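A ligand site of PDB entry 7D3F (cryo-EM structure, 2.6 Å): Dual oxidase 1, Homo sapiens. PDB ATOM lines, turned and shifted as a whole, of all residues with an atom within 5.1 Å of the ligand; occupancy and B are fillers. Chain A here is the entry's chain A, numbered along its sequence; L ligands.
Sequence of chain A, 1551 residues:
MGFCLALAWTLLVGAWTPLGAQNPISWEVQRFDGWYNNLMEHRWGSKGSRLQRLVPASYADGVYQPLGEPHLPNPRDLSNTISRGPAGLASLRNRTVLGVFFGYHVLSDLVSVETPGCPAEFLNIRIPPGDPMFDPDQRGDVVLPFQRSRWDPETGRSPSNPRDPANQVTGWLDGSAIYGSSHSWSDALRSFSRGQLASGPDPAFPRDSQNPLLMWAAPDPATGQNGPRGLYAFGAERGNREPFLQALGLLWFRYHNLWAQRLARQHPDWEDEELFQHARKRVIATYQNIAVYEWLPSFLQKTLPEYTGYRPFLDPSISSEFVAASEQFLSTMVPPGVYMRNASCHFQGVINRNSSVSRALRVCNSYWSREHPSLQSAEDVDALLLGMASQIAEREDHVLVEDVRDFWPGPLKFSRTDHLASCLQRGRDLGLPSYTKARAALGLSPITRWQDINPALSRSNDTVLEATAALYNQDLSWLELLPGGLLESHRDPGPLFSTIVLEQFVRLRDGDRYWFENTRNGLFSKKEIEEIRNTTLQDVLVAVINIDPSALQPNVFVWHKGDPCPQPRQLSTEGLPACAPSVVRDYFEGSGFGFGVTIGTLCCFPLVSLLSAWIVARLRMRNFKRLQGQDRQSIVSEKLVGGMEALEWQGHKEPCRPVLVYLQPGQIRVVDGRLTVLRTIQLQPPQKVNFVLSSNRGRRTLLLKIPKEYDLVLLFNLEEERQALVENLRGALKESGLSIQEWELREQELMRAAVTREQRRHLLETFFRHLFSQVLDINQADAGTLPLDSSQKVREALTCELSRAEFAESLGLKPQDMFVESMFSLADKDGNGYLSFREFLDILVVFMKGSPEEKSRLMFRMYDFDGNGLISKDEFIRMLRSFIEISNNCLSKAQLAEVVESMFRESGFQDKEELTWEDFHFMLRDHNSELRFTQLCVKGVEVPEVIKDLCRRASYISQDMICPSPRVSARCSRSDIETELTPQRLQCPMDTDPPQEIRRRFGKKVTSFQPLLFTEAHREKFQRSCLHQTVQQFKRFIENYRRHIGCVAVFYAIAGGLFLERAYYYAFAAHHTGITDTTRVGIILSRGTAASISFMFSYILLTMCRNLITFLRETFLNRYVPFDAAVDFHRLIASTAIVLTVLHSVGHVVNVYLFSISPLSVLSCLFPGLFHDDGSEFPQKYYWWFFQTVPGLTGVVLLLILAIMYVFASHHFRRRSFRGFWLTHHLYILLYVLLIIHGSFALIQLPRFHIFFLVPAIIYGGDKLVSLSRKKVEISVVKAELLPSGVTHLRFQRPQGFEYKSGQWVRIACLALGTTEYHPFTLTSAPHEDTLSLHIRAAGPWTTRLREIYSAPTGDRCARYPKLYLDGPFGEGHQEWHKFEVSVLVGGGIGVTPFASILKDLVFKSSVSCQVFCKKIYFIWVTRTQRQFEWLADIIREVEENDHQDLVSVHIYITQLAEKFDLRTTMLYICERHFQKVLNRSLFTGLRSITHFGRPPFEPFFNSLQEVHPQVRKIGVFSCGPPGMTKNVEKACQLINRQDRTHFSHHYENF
NH1 of Arg 1036 is in salt-bridge range of O17 of the ligand (2.5 Å). OG1 of Thr 1455 is in hydrogen-bond range of O5 of the ligand (2.6 Å). The guanidinium group of Arg 1495 is in salt-bridge range of an oxygen (O17) of the ligand (2.8 Å). N of Arg 1424 lies within hydrogen-bond range of O5 of the ligand (2.8 Å). NE of Arg 1424 lies within salt-bridge range of O15 of the ligand (2.8 Å). OE1 of Glu 1039 lies within hydrogen-bond range of N3 of the ligand (3.2 Å). OH of Tyr 1041 sits at hydrogen-bond distance from O12 of the ligand (3.3 Å). A nitrogen (N7) of the ligand sits at hydrogen-bond distance from the backbone carbonyl oxygen of Glu 1549, at 3.3 Å. A nitrogen (N2) of the ligand lies close to the side-chain amide oxygen of Asn 1040, at 3.4 Å. The side-chain sulfur (SG) of Cys 1520 lies within hydrogen-bond range of a nitrogen (N7) of the ligand (3.6 Å).
N of Thr 1455 sits at hydrogen-bond distance from O of Thr 1423, 2.8 Å away. The backbone carbonyl oxygen (O) of Arg 1424 sits close to the backbone NH (N) of Gln 1456 (3.4 Å). The side-chain amide oxygen of Asn 1528 sits close to the backbone carbonyl oxygen of Gly 1524. The side-chain sulfur (SG) of Cys 1520 sits close to the backbone carbonyl oxygen (O) of Glu 1549, 3.6 Å away. The backbone NH (N) of Gly 1389 sits at hydrogen-bond distance from the backbone carbonyl oxygen (O) of Val 1422, 3.3 Å away. The backbone carbonyl oxygen (O) of Gly 1391 lies within hydrogen-bond range of the side-chain sulfur (SG) of Cys 1520. The backbone NH of Gly 1388 sits at hydrogen-bond distance from the backbone carbonyl oxygen of Cys 1520 (3.1 Å). ND2 of Asn 1550 lies within hydrogen-bond range of OD1 of Asn 1118 (2.6 Å).
Residues that only touch the ligand: Gly 1388, Gly 1389, Ile 1390, Gly 1391, Thr 1423, Gly 1521, Pro 1522, Pro 1523, Gly 1524, Asn 1528 and Asn 1550. Hydrophobic or aromatic side chains within 4 Å of the ligand: Tyr 1041, Ile 1390, Pro 1522 and Pro 1523.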
ATOM      1  N   ARG A1036      31.733   3.881 -31.581  1.00  0.00           N
ATOM      2  CA  ARG A1036      30.657   3.043 -31.055  1.00  0.00           C
ATOM      3  C   ARG A1036      29.628   3.892 -30.320  1.00  0.00           C
ATOM      4  O   ARG A1036      28.419   3.736 -30.521  1.00  0.00           O
ATOM      5  CB  ARG A1036      31.222   1.966 -30.139  1.00  0.00           C
ATOM      6  CG  ARG A1036      30.186   1.254 -29.296  1.00  0.00           C
ATOM      7  CD  ARG A1036      29.243   0.433 -30.148  1.00  0.00           C
ATOM      8  NE  ARG A1036      29.958  -0.619 -30.868  1.00  0.00           N
ATOM      9  CZ  ARG A1036      30.224  -1.821 -30.358  1.00  0.00           C
ATOM     10  NH1 ARG A1036      30.872  -2.714 -31.082  1.00  0.00           N
ATOM     11  NH2 ARG A1036      29.831  -2.128 -29.130  1.00  0.00           N
ATOM     12  N   GLU A1039      27.659   5.988 -32.891  1.00  0.00           N
ATOM     13  CA  GLU A1039      26.781   5.159 -33.701  1.00  0.00           C
ATOM     14  C   GLU A1039      25.611   4.624 -32.883  1.00  0.00           C
ATOM     15  O   GLU A1039      24.541   4.362 -33.445  1.00  0.00           O
ATOM     16  CB  GLU A1039      27.573   4.007 -34.302  1.00  0.00           C
ATOM     17  CG  GLU A1039      26.828   3.223 -35.381  1.00  0.00           C
ATOM     18  CD  GLU A1039      27.682   2.133 -36.009  1.00  0.00           C
ATOM     19  OE1 GLU A1039      28.763   1.820 -35.462  1.00  0.00           O
ATOM     20  OE2 GLU A1039      27.268   1.591 -37.065  1.00  0.00           O
ATOM     21  N   ASN A1040      25.788   4.470 -31.572  1.00  0.00           N
ATOM     22  CA  ASN A1040      24.691   3.986 -30.743  1.00  0.00           C
ATOM     23  C   ASN A1040      23.759   5.106 -30.310  1.00  0.00           C
ATOM     24  O   ASN A1040      22.543   4.900 -30.208  1.00  0.00           O
ATOM     25  CB  ASN A1040      25.233   3.244 -29.525  1.00  0.00           C
ATOM     26  CG  ASN A1040      25.484   1.763 -29.806  1.00  0.00           C
ATOM     27  OD1 ASN A1040      25.424   1.319 -30.945  1.00  0.00           O
ATOM     28  ND2 ASN A1040      25.762   1.002 -28.748  1.00  0.00           N
ATOM     29  N   TYR A1041      24.286   6.300 -30.027  1.00  0.00           N
ATOM     30  CA  TYR A1041      23.498   7.382 -29.451  1.00  0.00           C
ATOM     31  C   TYR A1041      23.446   8.619 -30.339  1.00  0.00           C
ATOM     32  O   TYR A1041      23.378   9.734 -29.836  1.00  0.00           O
ATOM     33  CB  TYR A1041      24.026   7.738 -28.060  1.00  0.00           C
ATOM     34  CG  TYR A1041      23.940   6.619 -27.052  1.00  0.00           C
ATOM     35  CD1 TYR A1041      25.002   5.734 -26.888  1.00  0.00           C
ATOM     36  CD2 TYR A1041      22.815   6.451 -26.265  1.00  0.00           C
ATOM     37  CE1 TYR A1041      24.923   4.705 -25.962  1.00  0.00           C
ATOM     38  CE2 TYR A1041      22.728   5.432 -25.336  1.00  0.00           C
ATOM     39  CZ  TYR A1041      23.797   4.557 -25.184  1.00  0.00           C
ATOM     40  OH  TYR A1041      23.726   3.537 -24.271  1.00  0.00           O
ATOM     41  N   ARG A1043      20.941   9.469 -32.219  1.00  0.00           N
ATOM     42  CA  ARG A1043      19.625  10.061 -32.003  1.00  0.00           C
ATOM     43  C   ARG A1043      19.594  10.889 -30.727  1.00  0.00           C
ATOM     44  O   ARG A1043      19.060  12.011 -30.709  1.00  0.00           O
ATOM     45  CB  ARG A1043      18.560   8.961 -31.951  1.00  0.00           C
ATOM     46  CG  ARG A1043      18.460   8.109 -33.199  1.00  0.00           C
ATOM     47  CD  ARG A1043      17.471   6.979 -32.993  1.00  0.00           C
ATOM     48  NE  ARG A1043      17.865   6.104 -31.892  1.00  0.00           N
ATOM     49  CZ  ARG A1043      17.080   5.200 -31.320  1.00  0.00           C
ATOM     50  NH1 ARG A1043      15.833   5.050 -31.751  1.00  0.00           N
ATOM     51  NH2 ARG A1043      17.530   4.449 -30.326  1.00  0.00           N
ATOM     52  N   HIS A1044      20.160  10.355 -29.644  1.00  0.00           N
ATOM     53  CA  HIS A1044      20.217  11.091 -28.388  1.00  0.00           C
ATOM     54  C   HIS A1044      21.032  12.372 -28.535  1.00  0.00           C
ATOM     55  O   HIS A1044      20.637  13.437 -28.048  1.00  0.00           O
ATOM     56  CB  HIS A1044      20.813  10.221 -27.285  1.00  0.00           C
ATOM     57  CG  HIS A1044      20.181   8.867 -27.166  1.00  0.00           C
ATOM     58  ND1 HIS A1044      20.397   7.865 -28.087  1.00  0.00           N
ATOM     59  CD2 HIS A1044      19.355   8.350 -26.232  1.00  0.00           C
ATOM     60  CE1 HIS A1044      19.723   6.788 -27.734  1.00  0.00           C
ATOM     61  NE2 HIS A1044      19.073   7.056 -26.604  1.00  0.00           N
ATOM     62  N   ASN A1118      10.952   7.227 -34.465  1.00  0.00           N
ATOM     63  CA  ASN A1118      11.858   6.542 -33.554  1.00  0.00           C
ATOM     64  C   ASN A1118      13.251   6.384 -34.133  1.00  0.00           C
ATOM     65  O   ASN A1118      14.215   6.226 -33.377  1.00  0.00           O
ATOM     66  CB  ASN A1118      11.284   5.180 -33.180  1.00  0.00           C
ATOM     67  CG  ASN A1118      11.909   4.609 -31.929  1.00  0.00           C
ATOM     68  OD1 ASN A1118      12.920   3.892 -31.994  1.00  0.00           O
ATOM     69  ND2 ASN A1118      11.323   4.909 -30.775  1.00  0.00           N
ATOM     70  N   ASP A1124      12.358   6.004 -25.964  1.00  0.00           N
ATOM     71  CA  ASP A1124      12.529   5.175 -24.782  1.00  0.00           C
ATOM     72  C   ASP A1124      13.419   5.830 -23.731  1.00  0.00           C
ATOM     73  O   ASP A1124      13.358   5.443 -22.556  1.00  0.00           O
ATOM     74  CB  ASP A1124      13.115   3.805 -25.150  1.00  0.00           C
ATOM     75  CG  ASP A1124      12.125   2.939 -25.897  1.00  0.00           C
ATOM     76  OD1 ASP A1124      12.490   2.383 -26.951  1.00  0.00           O
ATOM     77  OD2 ASP A1124      10.969   2.816 -25.433  1.00  0.00           O
ATOM     78  N   GLY A1388      19.492  -8.138 -30.023  1.00  0.00           N
ATOM     79  CA  GLY A1388      20.724  -7.593 -29.489  1.00  0.00           C
ATOM     80  C   GLY A1388      20.548  -6.880 -28.162  1.00  0.00           C
ATOM     81  O   GLY A1388      19.692  -6.001 -28.034  1.00  0.00           O
ATOM     82  N   GLY A1389      21.368  -7.253 -27.172  1.00  0.00           N
ATOM     83  CA  GLY A1389      21.290  -6.601 -25.877  1.00  0.00           C
ATOM     84  C   GLY A1389      19.939  -6.791 -25.231  1.00  0.00           C
ATOM     85  O   GLY A1389      19.381  -7.902 -25.208  1.00  0.00           O
ATOM     86  N   ILE A1390      19.396  -5.699 -24.688  1.00  0.00           N
ATOM     87  CA  ILE A1390      18.080  -5.743 -24.057  1.00  0.00           C
ATOM     88  C   ILE A1390      16.949  -5.906 -25.057  1.00  0.00           C
ATOM     89  O   ILE A1390      15.810  -6.182 -24.646  1.00  0.00           O
ATOM     90  CB  ILE A1390      17.844  -4.477 -23.203  1.00  0.00           C
ATOM     91  CG1 ILE A1390      17.935  -3.227 -24.072  1.00  0.00           C
ATOM     92  CG2 ILE A1390      18.841  -4.418 -22.051  1.00  0.00           C
ATOM     93  CD1 ILE A1390      17.673  -1.937 -23.314  1.00  0.00           C
ATOM     94  N   GLY A1391      17.222  -5.735 -26.348  1.00  0.00           N
ATOM     95  CA  GLY A1391      16.204  -5.892 -27.361  1.00  0.00           C
ATOM     96  C   GLY A1391      15.970  -7.324 -27.764  1.00  0.00           C
ATOM     97  O   GLY A1391      15.639  -7.614 -28.919  1.00  0.00           O
ATOM     98  N   VAL A1422      22.402 -11.935 -30.380  1.00  0.00           N
ATOM     99  CA  VAL A1422      23.709 -11.307 -30.316  1.00  0.00           C
ATOM    100  C   VAL A1422      23.820 -10.588 -28.982  1.00  0.00           C
ATOM    101  O   VAL A1422      23.027  -9.687 -28.694  1.00  0.00           O
ATOM    102  CB  VAL A1422      23.945 -10.316 -31.469  1.00  0.00           C
ATOM    103  CG1 VAL A1422      25.362  -9.763 -31.430  1.00  0.00           C
ATOM    104  CG2 VAL A1422      23.669 -10.985 -32.812  1.00  0.00           C
ATOM    105  N   THR A1423      24.796 -10.980 -28.165  1.00  0.00           N
ATOM    106  CA  THR A1423      24.971 -10.338 -26.865  1.00  0.00           C
ATOM    107  C   THR A1423      26.439 -10.346 -26.477  1.00  0.00           C
ATOM    108  O   THR A1423      27.226 -11.175 -26.949  1.00  0.00           O
ATOM    109  CB  THR A1423      24.142 -11.026 -25.770  1.00  0.00           C
ATOM    110  OG1 THR A1423      23.860 -12.381 -26.155  1.00  0.00           O
ATOM    111  CG2 THR A1423      22.842 -10.275 -25.532  1.00  0.00           C
ATOM    112  N   ARG A1424      26.801  -9.404 -25.609  1.00  0.00           N
ATOM    113  CA  ARG A1424      28.134  -9.415 -25.012  1.00  0.00           C
ATOM    114  C   ARG A1424      28.263 -10.551 -24.018  1.00  0.00           C
ATOM    115  O   ARG A1424      29.095 -11.447 -24.182  1.00  0.00           O
ATOM    116  CB  ARG A1424      28.399  -8.068 -24.340  1.00  0.00           C
ATOM    117  CG  ARG A1424      29.785  -7.925 -23.733  1.00  0.00           C
ATOM    118  CD  ARG A1424      30.555  -6.798 -24.406  1.00  0.00           C
ATOM    119  NE  ARG A1424      29.692  -5.676 -24.736  1.00  0.00           N
ATOM    120  CZ  ARG A1424      29.342  -4.718 -23.891  1.00  0.00           C
ATOM    121  NH1 ARG A1424      29.792  -4.735 -22.638  1.00  0.00           N
ATOM    122  NH2 ARG A1424      28.546  -3.735 -24.290  1.00  0.00           N
ATOM    123  N   THR A1455      29.744 -11.730 -27.991  1.00  0.00           N
ATOM    124  CA  THR A1455      30.720 -10.799 -28.536  1.00  0.00           C
ATOM    125  C   THR A1455      31.700 -10.275 -27.486  1.00  0.00           C
ATOM    126  O   THR A1455      32.498  -9.394 -27.800  1.00  0.00           O
ATOM    127  CB  THR A1455      30.006  -9.614 -29.192  1.00  0.00           C
ATOM    128  OG1 THR A1455      29.132  -8.996 -28.242  1.00  0.00           O
ATOM    129  CG2 THR A1455      29.189 -10.087 -30.384  1.00  0.00           C
ATOM    130  N   GLN A1456      31.638 -10.784 -26.262  1.00  0.00           N
ATOM    131  CA  GLN A1456      32.564 -10.334 -25.220  1.00  0.00           C
ATOM    132  C   GLN A1456      33.990 -10.707 -25.576  1.00  0.00           C
ATOM    133  O   GLN A1456      34.253 -11.795 -26.107  1.00  0.00           O
ATOM    134  CB  GLN A1456      32.182 -10.945 -23.871  1.00  0.00           C
ATOM    135  CG  GLN A1456      33.101 -10.585 -22.715  1.00  0.00           C
ATOM    136  CD  GLN A1456      33.001  -9.123 -22.314  1.00  0.00           C
ATOM    137  OE1 GLN A1456      33.487  -8.243 -23.024  1.00  0.00           O
ATOM    138  NE2 GLN A1456      32.362  -8.866 -21.177  1.00  0.00           N
ATOM    139  N   ARG A1495      31.942 -11.411 -33.736  1.00  0.00           N
ATOM    140  CA  ARG A1495      30.912 -10.650 -34.427  1.00  0.00           C
ATOM    141  C   ARG A1495      30.134 -11.572 -35.355  1.00  0.00           C
ATOM    142  O   ARG A1495      30.745 -12.349 -36.106  1.00  0.00           O
ATOM    143  CB  ARG A1495      31.528  -9.504 -35.230  1.00  0.00           C
ATOM    144  CG  ARG A1495      32.713  -8.803 -34.571  1.00  0.00           C
ATOM    145  CD  ARG A1495      32.409  -8.336 -33.152  1.00  0.00           C
ATOM    146  NE  ARG A1495      31.169  -7.561 -33.067  1.00  0.00           N
ATOM    147  CZ  ARG A1495      30.750  -6.969 -31.964  1.00  0.00           C
ATOM    148  NH1 ARG A1495      31.464  -7.047 -30.856  1.00  0.00           N
ATOM    149  NH2 ARG A1495      29.610  -6.277 -31.965  1.00  0.00           N
ATOM    150  N   CYS A1520      15.984  -6.085 -33.904  1.00  0.00           N
ATOM    151  CA  CYS A1520      15.641  -5.391 -32.663  1.00  0.00           C
ATOM    152  C   CYS A1520      16.884  -5.432 -31.768  1.00  0.00           C
ATOM    153  O   CYS A1520      17.127  -6.420 -31.075  1.00  0.00           O
ATOM    154  CB  CYS A1520      14.438  -6.042 -31.975  1.00  0.00           C
ATOM    155  SG  CYS A1520      13.947  -5.251 -30.434  1.00  0.00           S
ATOM    156  N   GLY A1521      17.658  -4.357 -31.795  1.00  0.00           N
ATOM    157  CA  GLY A1521      18.877  -4.275 -31.024  1.00  0.00           C
ATOM    158  C   GLY A1521      19.448  -2.873 -31.019  1.00  0.00           C
ATOM    159  O   GLY A1521      18.755  -1.892 -31.323  1.00  0.00           O
ATOM    160  N   PRO A1522      20.723  -2.746 -30.660  1.00  0.00           N
ATOM    161  CA  PRO A1522      21.360  -1.433 -30.679  1.00  0.00           C
ATOM    162  C   PRO A1522      21.429  -0.895 -32.091  1.00  0.00           C
ATOM    163  O   PRO A1522      21.454  -1.671 -33.071  1.00  0.00           O
ATOM    164  CB  PRO A1522      22.757  -1.714 -30.112  1.00  0.00           C
ATOM    165  CG  PRO A1522      23.001  -3.143 -30.399  1.00  0.00           C
ATOM    166  CD  PRO A1522      21.664  -3.818 -30.268  1.00  0.00           C
ATOM    167  N   PRO A1523      21.444   0.433 -32.254  1.00  0.00           N
ATOM    168  CA  PRO A1523      21.417   1.003 -33.615  1.00  0.00           C
ATOM    169  C   PRO A1523      22.566   0.534 -34.486  1.00  0.00           C
ATOM    170  O   PRO A1523      22.377   0.347 -35.702  1.00  0.00           O
ATOM    171  CB  PRO A1523      21.492   2.515 -33.349  1.00  0.00           C
ATOM    172  CG  PRO A1523      20.936   2.680 -31.979  1.00  0.00           C
ATOM    173  CD  PRO A1523      21.387   1.476 -31.212  1.00  0.00           C
ATOM    174  N   GLY A1524      23.750   0.319 -33.915  1.00  0.00           N
ATOM    175  CA  GLY A1524      24.866  -0.167 -34.715  1.00  0.00           C
ATOM    176  C   GLY A1524      24.636  -1.569 -35.253  1.00  0.00           C
ATOM    177  O   GLY A1524      24.957  -1.867 -36.410  1.00  0.00           O
ATOM    178  N   MET A1525      24.091  -2.461 -34.420  1.00  0.00           N
ATOM    179  CA  MET A1525      23.840  -3.830 -34.868  1.00  0.00           C
ATOM    180  C   MET A1525      22.797  -3.863 -35.973  1.00  0.00           C
ATOM    181  O   MET A1525      22.969  -4.557 -36.984  1.00  0.00           O
ATOM    182  CB  MET A1525      23.400  -4.686 -33.678  1.00  0.00           C
ATOM    183  CG  MET A1525      23.244  -6.167 -34.013  1.00  0.00           C
ATOM    184  SD  MET A1525      21.909  -6.944 -33.090  1.00  0.00           S
ATOM    185  CE  MET A1525      20.494  -6.077 -33.775  1.00  0.00           C
ATOM    186  N   ASN A1528      24.324  -2.622 -39.144  1.00  0.00           N
ATOM    187  CA  ASN A1528      25.137  -3.656 -39.788  1.00  0.00           C
ATOM    188  C   ASN A1528      24.259  -4.676 -40.491  1.00  0.00           C
ATOM    189  O   ASN A1528      24.578  -5.126 -41.600  1.00  0.00           O
ATOM    190  CB  ASN A1528      26.038  -4.341 -38.761  1.00  0.00           C
ATOM    191  CG  ASN A1528      27.216  -3.477 -38.355  1.00  0.00           C
ATOM    192  OD1 ASN A1528      27.228  -2.269 -38.584  1.00  0.00           O
ATOM    193  ND2 ASN A1528      28.223  -4.103 -37.756  1.00  0.00           N
ATOM    194  N   GLU A1549      12.637  -3.158 -35.875  1.00  0.00           N
ATOM    195  CA  GLU A1549      11.597  -3.507 -34.912  1.00  0.00           C
ATOM    196  C   GLU A1549      11.970  -2.981 -33.540  1.00  0.00           C
ATOM    197  O   GLU A1549      13.126  -3.061 -33.112  1.00  0.00           O
ATOM    198  CB  GLU A1549      11.375  -5.022 -34.871  1.00  0.00           C
ATOM    199  CG  GLU A1549      10.738  -5.597 -36.122  1.00  0.00           C
ATOM    200  CD  GLU A1549       9.245  -5.295 -36.229  1.00  0.00           C
ATOM    201  OE1 GLU A1549       8.622  -5.752 -37.208  1.00  0.00           O
ATOM    202  OE2 GLU A1549       8.698  -4.616 -35.335  1.00  0.00           O
ATOM    203  N   ASN A1550      10.978  -2.439 -32.839  1.00  0.00           N
ATOM    204  CA  ASN A1550      11.163  -1.769 -31.551  1.00  0.00           C
ATOM    205  C   ASN A1550      10.121  -2.239 -30.550  1.00  0.00           C
ATOM    206  O   ASN A1550       9.424  -1.451 -29.909  1.00  0.00           O
ATOM    207  CB  ASN A1550      11.093  -0.249 -31.722  1.00  0.00           C
ATOM    208  CG  ASN A1550      11.688   0.493 -30.535  1.00  0.00           C
ATOM    209  OD1 ASN A1550      11.834  -0.061 -29.440  1.00  0.00           O
ATOM    210  ND2 ASN A1550      12.036   1.750 -30.750  1.00  0.00           N
HETATM  211  P1  LIG L   1      24.547  -4.165 -25.428  1.00  0.00           P
HETATM  212  O1  LIG L   1      24.817  -4.614 -24.011  1.00  0.00           O
HETATM  213  O2  LIG L   1      25.482  -3.179 -26.094  1.00  0.00           O
HETATM  214  O3  LIG L   1      24.436  -5.470 -26.366  1.00  0.00           O
HETATM  215  C1  LIG L   1      24.234  -5.302 -27.763  1.00  0.00           C
HETATM  216  C2  LIG L   1      25.105  -6.262 -28.558  1.00  0.00           C
HETATM  217  O4  LIG L   1      25.293  -5.718 -29.860  1.00  0.00           O
HETATM  218  C3  LIG L   1      26.467  -6.357 -27.900  1.00  0.00           C
HETATM  219  O5  LIG L   1      26.893  -7.728 -27.864  1.00  0.00           O
HETATM  220  C4  LIG L   1      27.402  -5.572 -28.794  1.00  0.00           C
HETATM  221  O6  LIG L   1      28.652  -6.247 -28.919  1.00  0.00           O
HETATM  222  C5  LIG L   1      26.671  -5.441 -30.114  1.00  0.00           C
HETATM  223  N1  LIG L   1      26.817  -4.037 -30.595  1.00  0.00           N
HETATM  224  C6  LIG L   1      26.481  -2.940 -29.896  1.00  0.00           C
HETATM  225  N2  LIG L   1      26.733  -1.811 -30.609  1.00  0.00           N
HETATM  226  C7  LIG L   1      27.246  -2.193 -31.796  1.00  0.00           C
HETATM  227  C8  LIG L   1      27.721  -1.503 -33.013  1.00  0.00           C
HETATM  228  N3  LIG L   1      27.717  -0.153 -33.106  1.00  0.00           N
HETATM  229  N4  LIG L   1      28.177  -2.272 -34.029  1.00  0.00           N
HETATM  230  C9  LIG L   1      28.197  -3.614 -33.952  1.00  0.00           C
HETATM  231  N5  LIG L   1      27.774  -4.300 -32.876  1.00  0.00           N
HETATM  232  C10 LIG L   1      27.297  -3.660 -31.774  1.00  0.00           C
HETATM  233  O7  LIG L   1      23.052  -3.581 -25.514  1.00  0.00           O
HETATM  234  P2  LIG L   1      22.660  -2.266 -24.673  1.00  0.00           P
HETATM  235  O8  LIG L   1      21.536  -2.636 -23.737  1.00  0.00           O
HETATM  236  O9  LIG L   1      23.927  -1.645 -24.126  1.00  0.00           O
HETATM  237  O10 LIG L   1      22.065  -1.296 -25.814  1.00  0.00           O
HETATM  238  C11 LIG L   1      22.612   0.008 -25.982  1.00  0.00           C
HETATM  239  C12 LIG L   1      21.525   0.967 -26.461  1.00  0.00           C
HETATM  240  O11 LIG L   1      20.785   0.383 -27.534  1.00  0.00           O
HETATM  241  C13 LIG L   1      20.540   1.255 -25.332  1.00  0.00           C
HETATM  242  O12 LIG L   1      20.664   2.619 -24.919  1.00  0.00           O
HETATM  243  C14 LIG L   1      19.166   1.009 -25.926  1.00  0.00           C
HETATM  244  O13 LIG L   1      18.354   2.175 -25.769  1.00  0.00           O
HETATM  245  C15 LIG L   1      19.404   0.721 -27.392  1.00  0.00           C
HETATM  246  N6  LIG L   1      18.538  -0.382 -27.818  1.00  0.00           N
HETATM  247  C16 LIG L   1      17.544  -0.129 -28.677  1.00  0.00           C
HETATM  248  C17 LIG L   1      16.684  -1.132 -29.122  1.00  0.00           C
HETATM  249  C18 LIG L   1      15.585  -0.786 -30.081  1.00  0.00           C
HETATM  250  O14 LIG L   1      15.395   0.386 -30.365  1.00  0.00           O
HETATM  251  N7  LIG L   1      14.854  -1.764 -30.597  1.00  0.00           N
HETATM  252  C19 LIG L   1      16.848  -2.553 -28.652  1.00  0.00           C
HETATM  253  C20 LIG L   1      17.969  -2.700 -27.735  1.00  0.00           C
HETATM  254  C21 LIG L   1      18.754  -1.617 -27.357  1.00  0.00           C
HETATM  255  P3  LIG L   1      29.999  -5.504 -28.465  1.00  0.00           P
HETATM  256  O15 LIG L   1      29.564  -4.618 -27.325  1.00  0.00           O
HETATM  257  O16 LIG L   1      30.917  -6.634 -28.057  1.00  0.00           O
HETATM  258  O17 LIG L   1      30.433  -4.759 -29.699  1.00  0.00           O
